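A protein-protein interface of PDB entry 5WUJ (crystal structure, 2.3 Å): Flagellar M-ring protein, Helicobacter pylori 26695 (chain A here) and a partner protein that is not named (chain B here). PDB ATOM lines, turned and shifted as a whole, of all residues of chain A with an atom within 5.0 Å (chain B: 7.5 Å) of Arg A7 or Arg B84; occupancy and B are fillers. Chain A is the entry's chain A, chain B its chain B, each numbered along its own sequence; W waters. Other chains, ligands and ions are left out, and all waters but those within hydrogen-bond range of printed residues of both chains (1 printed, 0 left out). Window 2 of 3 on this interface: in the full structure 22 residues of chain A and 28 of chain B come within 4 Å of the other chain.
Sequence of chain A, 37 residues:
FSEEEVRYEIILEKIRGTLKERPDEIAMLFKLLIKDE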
ATOM      1  N   SER A   2     -21.038  15.800 -18.046  1.00  0.00           N
ATOM      2  CA  SER A   2     -21.301  14.736 -19.002  1.00  0.00           C
ATOM      3  C   SER A   2     -20.006  14.058 -19.440  1.00  0.00           C
ATOM      4  O   SER A   2     -18.902  14.611 -19.317  1.00  0.00           O
ATOM      5  CB  SER A   2     -22.003  15.302 -20.233  1.00  0.00           C
ATOM      6  OG  SER A   2     -21.226  16.355 -20.798  1.00  0.00           O
ATOM      7  N   GLU A   3     -20.153  12.842 -19.978  1.00  0.00           N
ATOM      8  CA  GLU A   3     -19.004  12.134 -20.533  1.00  0.00           C
ATOM      9  C   GLU A   3     -18.311  12.971 -21.611  1.00  0.00           C
ATOM     10  O   GLU A   3     -17.078  12.996 -21.695  1.00  0.00           O
ATOM     11  CB  GLU A   3     -19.441  10.786 -21.111  1.00  0.00           C
ATOM     12  CG  GLU A   3     -18.334  10.077 -21.891  1.00  0.00           C
ATOM     13  CD  GLU A   3     -18.842   8.954 -22.786  1.00  0.00           C
ATOM     14  OE1 GLU A   3     -20.075   8.782 -22.882  1.00  0.00           O
ATOM     15  OE2 GLU A   3     -18.004   8.236 -23.377  1.00  0.00           O
ATOM     16  N   GLU A   4     -19.099  13.668 -22.432  1.00  0.00           N
ATOM     17  CA  GLU A   4     -18.552  14.536 -23.467  1.00  0.00           C
ATOM     18  C   GLU A   4     -17.745  15.671 -22.852  1.00  0.00           C
ATOM     19  O   GLU A   4     -16.638  15.973 -23.303  1.00  0.00           O
ATOM     20  CB  GLU A   4     -19.684  15.103 -24.330  1.00  0.00           C
ATOM     21  CG  GLU A   4     -20.440  14.076 -25.158  1.00  0.00           C
ATOM     22  CD  GLU A   4     -21.555  13.378 -24.380  1.00  0.00           C
ATOM     23  OE1 GLU A   4     -22.048  13.936 -23.374  1.00  0.00           O
ATOM     24  OE2 GLU A   4     -21.942  12.261 -24.785  1.00  0.00           O
ATOM     25  N   GLU A   5     -18.298  16.321 -21.825  1.00  0.00           N
ATOM     26  CA  GLU A   5     -17.590  17.426 -21.194  1.00  0.00           C
ATOM     27  C   GLU A   5     -16.295  16.945 -20.546  1.00  0.00           C
ATOM     28  O   GLU A   5     -15.258  17.611 -20.641  1.00  0.00           O
ATOM     29  CB  GLU A   5     -18.502  18.121 -20.178  1.00  0.00           C
ATOM     30  CG  GLU A   5     -17.861  19.253 -19.394  1.00  0.00           C
ATOM     31  CD  GLU A   5     -17.213  20.307 -20.290  1.00  0.00           C
ATOM     32  OE1 GLU A   5     -16.148  20.850 -19.906  1.00  0.00           O
ATOM     33  OE2 GLU A   5     -17.773  20.593 -21.373  1.00  0.00           O
ATOM     34  N   VAL A   6     -16.318  15.753 -19.944  1.00  0.00           N
ATOM     35  CA  VAL A   6     -15.133  15.228 -19.281  1.00  0.00           C
ATOM     36  C   VAL A   6     -14.081  14.823 -20.311  1.00  0.00           C
ATOM     37  O   VAL A   6     -12.881  15.034 -20.105  1.00  0.00           O
ATOM     38  CB  VAL A   6     -15.517  14.052 -18.371  1.00  0.00           C
ATOM     39  CG1 VAL A   6     -14.285  13.330 -17.938  1.00  0.00           C
ATOM     40  CG2 VAL A   6     -16.331  14.539 -17.160  1.00  0.00           C
ATOM     41  N   ARG A   7     -14.509  14.232 -21.432  1.00  0.00           N
ATOM     42  CA  ARG A   7     -13.546  13.831 -22.458  1.00  0.00           C
ATOM     43  C   ARG A   7     -12.880  15.048 -23.077  1.00  0.00           C
ATOM     44  O   ARG A   7     -11.657  15.065 -23.266  1.00  0.00           O
ATOM     45  CB  ARG A   7     -14.232  12.990 -23.539  1.00  0.00           C
ATOM     46  CG  ARG A   7     -14.636  11.591 -23.049  1.00  0.00           C
ATOM     47  CD  ARG A   7     -15.405  10.816 -24.115  1.00  0.00           C
ATOM     48  NE  ARG A   7     -14.625  10.684 -25.340  1.00  0.00           N
ATOM     49  CZ  ARG A   7     -15.124  10.319 -26.514  1.00  0.00           C
ATOM     50  NH1 ARG A   7     -16.413  10.040 -26.634  1.00  0.00           N
ATOM     51  NH2 ARG A   7     -14.326  10.227 -27.565  1.00  0.00           N
ATOM     52  N   TYR A   8     -13.679  16.074 -23.380  1.00  0.00           N
ATOM     53  CA  TYR A   8     -13.151  17.366 -23.789  1.00  0.00           C
ATOM     54  C   TYR A   8     -12.053  17.832 -22.832  1.00  0.00           C
ATOM     55  O   TYR A   8     -10.966  18.224 -23.261  1.00  0.00           O
ATOM     56  CB  TYR A   8     -14.294  18.384 -23.846  1.00  0.00           C
ATOM     57  CG  TYR A   8     -13.843  19.783 -24.184  1.00  0.00           C
ATOM     58  CD1 TYR A   8     -13.539  20.699 -23.187  1.00  0.00           C
ATOM     59  CD2 TYR A   8     -13.724  20.183 -25.504  1.00  0.00           C
ATOM     60  CE1 TYR A   8     -13.108  21.988 -23.498  1.00  0.00           C
ATOM     61  CE2 TYR A   8     -13.303  21.454 -25.828  1.00  0.00           C
ATOM     62  CZ  TYR A   8     -12.998  22.354 -24.822  1.00  0.00           C
ATOM     63  OH  TYR A   8     -12.580  23.620 -25.144  1.00  0.00           O
ATOM     64  N   GLU A   9     -12.316  17.773 -21.524  1.00  0.00           N
ATOM     65  CA  GLU A   9     -11.325  18.227 -20.547  1.00  0.00           C
ATOM     66  C   GLU A   9     -10.084  17.355 -20.551  1.00  0.00           C
ATOM     67  O   GLU A   9      -8.981  17.850 -20.274  1.00  0.00           O
ATOM     68  CB  GLU A   9     -11.923  18.256 -19.138  1.00  0.00           C
ATOM     69  CG  GLU A   9     -13.040  19.273 -18.948  1.00  0.00           C
ATOM     70  CD  GLU A   9     -12.575  20.712 -19.149  1.00  0.00           C
ATOM     71  OE1 GLU A   9     -11.403  21.035 -18.820  1.00  0.00           O
ATOM     72  OE2 GLU A   9     -13.390  21.519 -19.642  1.00  0.00           O
ATOM     73  N   ILE A  10     -10.227  16.062 -20.859  1.00  0.00           N
ATOM     74  CA  ILE A  10      -9.043  15.204 -20.952  1.00  0.00           C
ATOM     75  C   ILE A  10      -8.110  15.694 -22.058  1.00  0.00           C
ATOM     76  O   ILE A  10      -6.909  15.876 -21.839  1.00  0.00           O
ATOM     77  CB  ILE A  10      -9.434  13.736 -21.172  1.00  0.00           C
ATOM     78  CG1 ILE A  10     -10.036  13.144 -19.900  1.00  0.00           C
ATOM     79  CG2 ILE A  10      -8.197  12.918 -21.564  1.00  0.00           C
ATOM     80  CD1 ILE A  10     -10.470  11.718 -20.081  1.00  0.00           C
ATOM     81  N   ILE A  11      -8.630  15.893 -23.274  1.00  0.00           N
ATOM     82  CA  ILE A  11      -7.714  16.258 -24.344  1.00  0.00           C
ATOM     83  C   ILE A  11      -7.227  17.697 -24.168  1.00  0.00           C
ATOM     84  O   ILE A  11      -6.051  17.986 -24.396  1.00  0.00           O
ATOM     85  CB  ILE A  11      -8.326  15.993 -25.736  1.00  0.00           C
ATOM     86  CG1 ILE A  11      -9.514  16.894 -26.045  1.00  0.00           C
ATOM     87  CG2 ILE A  11      -8.682  14.488 -25.892  1.00  0.00           C
ATOM     88  CD1 ILE A  11     -10.155  16.573 -27.404  1.00  0.00           C
ATOM     89  N   LEU B  62      -9.766  20.360 -31.287  1.00  0.00           N
ATOM     90  CA  LEU B  62      -8.875  19.748 -30.303  1.00  0.00           C
ATOM     91  C   LEU B  62      -8.647  18.275 -30.604  1.00  0.00           C
ATOM     92  O   LEU B  62      -7.526  17.769 -30.479  1.00  0.00           O
ATOM     93  CB  LEU B  62      -9.454  19.897 -28.898  1.00  0.00           C
ATOM     94  CG  LEU B  62      -9.475  21.294 -28.333  1.00  0.00           C
ATOM     95  CD1 LEU B  62      -9.837  21.239 -26.847  1.00  0.00           C
ATOM     96  CD2 LEU B  62      -8.136  21.989 -28.587  1.00  0.00           C
ATOM     97  N   GLU B  63      -9.706  17.565 -30.992  1.00  0.00           N
ATOM     98  CA  GLU B  63      -9.545  16.152 -31.319  1.00  0.00           C
ATOM     99  C   GLU B  63      -8.599  15.975 -32.496  1.00  0.00           C
ATOM    100  O   GLU B  63      -7.817  15.015 -32.543  1.00  0.00           O
ATOM    101  CB  GLU B  63     -10.898  15.520 -31.636  1.00  0.00           C
ATOM    102  CG  GLU B  63     -11.759  15.234 -30.424  1.00  0.00           C
ATOM    103  CD  GLU B  63     -12.853  14.227 -30.736  1.00  0.00           C
ATOM    104  OE1 GLU B  63     -13.038  13.911 -31.938  1.00  0.00           O
ATOM    105  OE2 GLU B  63     -13.513  13.746 -29.784  1.00  0.00           O
ATOM    106  N   GLY B  78      -2.866   9.286 -22.187  1.00  0.00           N
ATOM    107  CA  GLY B  78      -4.232   9.319 -22.678  1.00  0.00           C
ATOM    108  C   GLY B  78      -4.508   8.411 -23.859  1.00  0.00           C
ATOM    109  O   GLY B  78      -5.392   8.713 -24.671  1.00  0.00           O
ATOM    110  N   GLY B  79      -3.779   7.296 -23.975  1.00  0.00           N
ATOM    111  CA  GLY B  79      -4.037   6.370 -25.065  1.00  0.00           C
ATOM    112  C   GLY B  79      -5.461   5.840 -25.098  1.00  0.00           C
ATOM    113  O   GLY B  79      -6.010   5.597 -26.178  1.00  0.00           O
ATOM    114  N   LEU B  80      -6.085   5.667 -23.924  1.00  0.00           N
ATOM    115  CA  LEU B  80      -7.455   5.157 -23.876  1.00  0.00           C
ATOM    116  C   LEU B  80      -8.418   6.094 -24.606  1.00  0.00           C
ATOM    117  O   LEU B  80      -9.240   5.651 -25.416  1.00  0.00           O
ATOM    118  CB  LEU B  80      -7.884   4.961 -22.417  1.00  0.00           C
ATOM    119  CG  LEU B  80      -8.803   3.814 -22.006  1.00  0.00           C
ATOM    120  CD1 LEU B  80      -8.363   2.482 -22.622  1.00  0.00           C
ATOM    121  CD2 LEU B  80      -8.870   3.707 -20.478  1.00  0.00           C
ATOM    122  N   GLU B  81      -8.329   7.400 -24.326  1.00  0.00           N
ATOM    123  CA  GLU B  81      -9.178   8.385 -24.989  1.00  0.00           C
ATOM    124  C   GLU B  81      -8.857   8.491 -26.473  1.00  0.00           C
ATOM    125  O   GLU B  81      -9.754   8.736 -27.292  1.00  0.00           O
ATOM    126  CB  GLU B  81      -8.997   9.746 -24.308  1.00  0.00           C
ATOM    127  CG  GLU B  81      -9.667  10.946 -24.977  1.00  0.00           C
ATOM    128  CD  GLU B  81     -11.165  10.758 -25.237  1.00  0.00           C
ATOM    129  OE1 GLU B  81     -11.686  11.400 -26.178  1.00  0.00           O
ATOM    130  OE2 GLU B  81     -11.828   9.990 -24.501  1.00  0.00           O
ATOM    131  N   TYR B  82      -7.582   8.331 -26.836  1.00  0.00           N
ATOM    132  CA  TYR B  82      -7.220   8.313 -28.244  1.00  0.00           C
ATOM    133  C   TYR B  82      -7.846   7.113 -28.949  1.00  0.00           C
ATOM    134  O   TYR B  82      -8.428   7.245 -30.038  1.00  0.00           O
ATOM    135  CB  TYR B  82      -5.690   8.301 -28.388  1.00  0.00           C
ATOM    136  CG  TYR B  82      -5.237   8.237 -29.824  1.00  0.00           C
ATOM    137  CD1 TYR B  82      -5.629   9.212 -30.740  1.00  0.00           C
ATOM    138  CD2 TYR B  82      -4.435   7.196 -30.278  1.00  0.00           C
ATOM    139  CE1 TYR B  82      -5.220   9.160 -32.067  1.00  0.00           C
ATOM    140  CE2 TYR B  82      -4.022   7.140 -31.599  1.00  0.00           C
ATOM    141  CZ  TYR B  82      -4.419   8.123 -32.486  1.00  0.00           C
ATOM    142  OH  TYR B  82      -4.016   8.063 -33.799  1.00  0.00           O
ATOM    143  N   ALA B  83      -7.718   5.924 -28.351  1.00  0.00           N
ATOM    144  CA  ALA B  83      -8.403   4.742 -28.881  1.00  0.00           C
ATOM    145  C   ALA B  83      -9.903   4.983 -29.014  1.00  0.00           C
ATOM    146  O   ALA B  83     -10.509   4.658 -30.045  1.00  0.00           O
ATOM    147  CB  ALA B  83      -8.140   3.540 -27.974  1.00  0.00           C
ATOM    148  N   ARG B  84     -10.511   5.564 -27.979  1.00  0.00           N
ATOM    149  CA  ARG B  84     -11.950   5.811 -27.986  1.00  0.00           C
ATOM    150  C   ARG B  84     -12.353   6.695 -29.162  1.00  0.00           C
ATOM    151  O   ARG B  84     -13.362   6.432 -29.829  1.00  0.00           O
ATOM    152  CB  ARG B  84     -12.347   6.447 -26.652  1.00  0.00           C
ATOM    153  CG  ARG B  84     -13.825   6.446 -26.318  1.00  0.00           C
ATOM    154  CD  ARG B  84     -14.056   7.155 -24.975  1.00  0.00           C
ATOM    155  NE  ARG B  84     -13.721   6.309 -23.826  1.00  0.00           N
ATOM    156  CZ  ARG B  84     -12.745   6.555 -22.943  1.00  0.00           C
ATOM    157  NH1 ARG B  84     -11.975   7.635 -23.053  1.00  0.00           N
ATOM    158  NH2 ARG B  84     -12.535   5.707 -21.934  1.00  0.00           N
ATOM    159  N   GLU B  85     -11.572   7.747 -29.436  1.00  0.00           N
ATOM    160  CA  GLU B  85     -11.849   8.611 -30.583  1.00  0.00           C
ATOM    161  C   GLU B  85     -11.632   7.877 -31.899  1.00  0.00           C
ATOM    162  O   GLU B  85     -12.445   7.993 -32.824  1.00  0.00           O
ATOM    163  CB  GLU B  85     -10.962   9.855 -30.537  1.00  0.00           C
ATOM    164  CG  GLU B  85     -11.244  10.770 -29.365  1.00  0.00           C
ATOM    165  CD  GLU B  85     -10.202  11.879 -29.216  1.00  0.00           C
ATOM    166  OE1 GLU B  85      -9.393  12.080 -30.148  1.00  0.00           O
ATOM    167  OE2 GLU B  85     -10.190  12.542 -28.161  1.00  0.00           O
ATOM    168  N   LEU B  86     -10.534   7.124 -31.997  1.00  0.00           N
ATOM    169  CA  LEU B  86     -10.246   6.365 -33.211  1.00  0.00           C
ATOM    170  C   LEU B  86     -11.348   5.348 -33.514  1.00  0.00           C
ATOM    171  O   LEU B  86     -11.843   5.265 -34.647  1.00  0.00           O
ATOM    172  CB  LEU B  86      -8.904   5.659 -33.058  1.00  0.00           C
ATOM    173  CG  LEU B  86      -8.491   4.723 -34.193  1.00  0.00           C
ATOM    174  CD1 LEU B  86      -8.296   5.520 -35.480  1.00  0.00           C
ATOM    175  CD2 LEU B  86      -7.213   3.971 -33.831  1.00  0.00           C
ATOM    176  N   LEU B  87     -11.720   4.536 -32.517  1.00  0.00           N
ATOM    177  CA  LEU B  87     -12.703   3.478 -32.750  1.00  0.00           C
ATOM    178  C   LEU B  87     -14.078   4.056 -33.049  1.00  0.00           C
ATOM    179  O   LEU B  87     -14.826   3.500 -33.862  1.00  0.00           O
ATOM    180  CB  LEU B  87     -12.763   2.549 -31.544  1.00  0.00           C
ATOM    181  CG  LEU B  87     -11.449   1.796 -31.350  1.00  0.00           C
ATOM    182  CD1 LEU B  87     -11.263   1.338 -29.910  1.00  0.00           C
ATOM    183  CD2 LEU B  87     -11.357   0.619 -32.315  1.00  0.00           C
ATOM    184  N   THR B  88     -14.416   5.182 -32.428  1.00  0.00           N
ATOM    185  CA  THR B  88     -15.678   5.837 -32.741  1.00  0.00           C
ATOM    186  C   THR B  88     -15.698   6.331 -34.184  1.00  0.00           C
ATOM    187  O   THR B  88     -16.719   6.229 -34.872  1.00  0.00           O
ATOM    188  CB  THR B  88     -15.910   6.984 -31.757  1.00  0.00           C
ATOM    189  OG1 THR B  88     -15.987   6.447 -30.430  1.00  0.00           O
ATOM    190  CG2 THR B  88     -17.188   7.729 -32.080  1.00  0.00           C
ATOM    191  N   ARG B  89     -14.582   6.869 -34.666  1.00  0.00           N
ATOM    192  CA  ARG B  89     -14.546   7.305 -36.057  1.00  0.00           C
ATOM    193  C   ARG B  89     -14.636   6.118 -37.008  1.00  0.00           C
ATOM    194  O   ARG B  89     -15.300   6.196 -38.046  1.00  0.00           O
ATOM    195  CB  ARG B  89     -13.278   8.106 -36.332  1.00  0.00           C
ATOM    196  CG  ARG B  89     -13.332   9.528 -35.818  1.00  0.00           C
ATOM    197  CD  ARG B  89     -12.283  10.392 -36.501  1.00  0.00           C
ATOM    198  NE  ARG B  89     -10.928   9.935 -36.209  1.00  0.00           N
ATOM    199  CZ  ARG B  89     -10.228  10.297 -35.136  1.00  0.00           C
ATOM    200  NH1 ARG B  89     -10.753  11.128 -34.241  1.00  0.00           N
ATOM    201  NH2 ARG B  89      -9.001   9.825 -34.957  1.00  0.00           N
ATOM    202  N   THR B  90     -13.994   5.003 -36.662  1.00  0.00           N
ATOM    203  CA  THR B  90     -13.897   3.899 -37.600  1.00  0.00           C
ATOM    204  C   THR B  90     -15.040   2.902 -37.461  1.00  0.00           C
ATOM    205  O   THR B  90     -15.486   2.348 -38.470  1.00  0.00           O
ATOM    206  CB  THR B  90     -12.545   3.199 -37.432  1.00  0.00           C
ATOM    207  OG1 THR B  90     -12.303   2.938 -36.048  1.00  0.00           O
ATOM    208  CG2 THR B  90     -11.436   4.109 -37.956  1.00  0.00           C
ATOM    209  N   GLY B  92     -18.020   3.552 -35.372  1.00  0.00           N
ATOM    210  CA  GLY B  92     -19.237   4.109 -34.825  1.00  0.00           C
ATOM    211  C   GLY B  92     -19.332   3.902 -33.322  1.00  0.00           C
ATOM    212  O   GLY B  92     -18.642   3.069 -32.733  1.00  0.00           O
ATOM    213  N   SER B  93     -20.236   4.669 -32.704  1.00  0.00           N
ATOM    214  CA  SER B  93     -20.265   4.783 -31.245  1.00  0.00           C
ATOM    215  C   SER B  93     -20.472   3.436 -30.558  1.00  0.00           C
ATOM    216  O   SER B  93     -19.822   3.140 -29.547  1.00  0.00           O
ATOM    217  CB  SER B  93     -21.365   5.754 -30.818  1.00  0.00           C
ATOM    218  OG  SER B  93     -20.872   7.076 -30.729  1.00  0.00           O
ATOM    219  N   ALA B  96     -17.716   0.629 -31.085  1.00  0.00           N
ATOM    220  CA  ALA B  96     -16.505   1.114 -30.425  1.00  0.00           C
ATOM    221  C   ALA B  96     -16.570   0.893 -28.916  1.00  0.00           C
ATOM    222  O   ALA B  96     -15.559   0.554 -28.289  1.00  0.00           O
ATOM    223  CB  ALA B  96     -16.282   2.594 -30.732  1.00  0.00           C
ATOM    224  N   LYS B  97     -17.751   1.067 -28.314  1.00  0.00           N
ATOM    225  CA  LYS B  97     -17.856   0.874 -26.871  1.00  0.00           C
ATOM    226  C   LYS B  97     -17.596  -0.582 -26.490  1.00  0.00           C
ATOM    227  O   LYS B  97     -16.961  -0.861 -25.467  1.00  0.00           O
ATOM    228  CB  LYS B  97     -19.219   1.354 -26.361  1.00  0.00           C
ATOM    229  CG  LYS B  97     -19.566   0.813 -24.996  1.00  0.00           C
ATOM    230  CD  LYS B  97     -19.710   1.920 -23.963  1.00  0.00           C
ATOM    231  CE  LYS B  97     -19.471   1.400 -22.548  1.00  0.00           C
ATOM    232  NZ  LYS B  97     -18.755   2.387 -21.683  1.00  0.00           N
ATOM    233  N   MET B 100     -14.053  -0.862 -26.644  1.00  0.00           N
ATOM    234  CA  MET B 100     -13.463  -0.104 -25.546  1.00  0.00           C
ATOM    235  C   MET B 100     -13.540  -0.866 -24.226  1.00  0.00           C
ATOM    236  O   MET B 100     -12.565  -0.897 -23.465  1.00  0.00           O
ATOM    237  CB  MET B 100     -14.133   1.263 -25.419  1.00  0.00           C
ATOM    238  CG  MET B 100     -13.685   2.214 -26.511  1.00  0.00           C
ATOM    239  SD  MET B 100     -11.909   2.521 -26.453  1.00  0.00           S
ATOM    240  CE  MET B 100     -11.746   3.022 -24.731  1.00  0.00           C
ATOM    241  N   LEU B 103     -11.011  -3.297 -24.338  1.00  0.00           N
ATOM    242  CA  LEU B 103      -9.702  -2.651 -24.373  1.00  0.00           C
ATOM    243  C   LEU B 103      -9.245  -2.226 -22.982  1.00  0.00           C
ATOM    244  O   LEU B 103      -8.047  -2.288 -22.673  1.00  0.00           O
ATOM    245  CB  LEU B 103      -9.743  -1.444 -25.313  1.00  0.00           C
ATOM    246  CG  LEU B 103      -8.443  -0.928 -25.917  1.00  0.00           C
ATOM    247  CD1 LEU B 103      -7.515  -2.061 -26.290  1.00  0.00           C
ATOM    248  CD2 LEU B 103      -8.764  -0.112 -27.148  1.00  0.00           C
ATOM    249  N   THR B 104     -10.177  -1.767 -22.137  1.00  0.00           N
ATOM    250  CA  THR B 104      -9.814  -1.352 -20.782  1.00  0.00           C
ATOM    251  C   THR B 104      -9.410  -2.547 -19.920  1.00  0.00           C
ATOM    252  O   THR B 104      -8.491  -2.438 -19.101  1.00  0.00           O
ATOM    253  CB  THR B 104     -10.968  -0.575 -20.139  1.00  0.00           C
ATOM    254  OG1 THR B 104     -11.548   0.311 -21.107  1.00  0.00           O
ATOM    255  CG2 THR B 104     -10.481   0.227 -18.946  1.00  0.00           C
HETATM  256  O   HOH W   1     -17.469   7.233 -28.201  1.00  0.00           O
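The side-chain carboxylate of Glu B81 is in salt-bridge range of the guanidinium group of Arg A7 (3.0 Å).
The side-chain hydroxyl of Thr B88 is in hydrogen-bond range of the backbone carbonyl oxygen of Arg B84, 2.7 Å away. The backbone NH (N) of Arg B84 sits close to the side-chain sulfur (SD) of Met B100, 3.7 Å away. The side-chain carboxylate of Glu B85 lies close to the side-chain carboxylate of Glu B81. NH1 of Arg B84 lies within salt-bridge range of OE2 of Glu B81 (2.8 Å).
Among the printed residues, pairs that only touch across the chains: Ile A11 with Glu B85 (3.3 Å), Arg A7 with Arg B84 (3.6 Å), Arg A7 with Glu B85 (3.6 Å), Tyr A8 with Leu B62 (3.6 Å), Ile A11 with Glu B63 (3.7 Å), Ile A11 with Leu B62 (3.7 Å) and Ile A11 with Glu B81 (3.8 Å).
Arg A7 touches just these residues of chain B: Glu B81 (3.0 Å), Arg B84 (3.6 Å) and Glu B85 (3.6 Å). Arg B84 touches just one residue of chain A: Arg A7 (3.6 Å). Of the printed residues of chain A, Glu B63 touches Ile A11 (3.7 Å). Of the printed residues of chain B, Tyr A8 touches Leu B62 (3.6 Å). Of the printed residues of chain A, Glu B85 touches Arg A7 (3.6 Å) and Ile A11 (3.3 Å). Tyr B82 touches none of the printed residues of chain A. The nearest residue of chain B that does not touch Arg A7 is Glu B63 (4.2 Å). The nearest printed residue of chain B that does not touch Tyr A8 is Glu B81 (5.8 Å).
Of the 10 printed residues of chain A, 3 touch a printed residue of chain B. Hydrophobic or aromatic side chains of chain A within 4 Å of the printed part of chain B: Tyr A8 and Ile A11. Hydrophobic or aromatic side chains of chain B within 4 Å of the printed part of chain A: Leu B62. Among the printed residues, Asp or Glu carboxylates within 4 Å of a Lys or Arg side-chain nitrogen of the other chain: Arg A7 with Glu B81.
Water W1 bridges the side-chain hydroxyl of Thr B88 (2.8 Å) and the guanidinium group of Arg A7 (3.4 Å).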
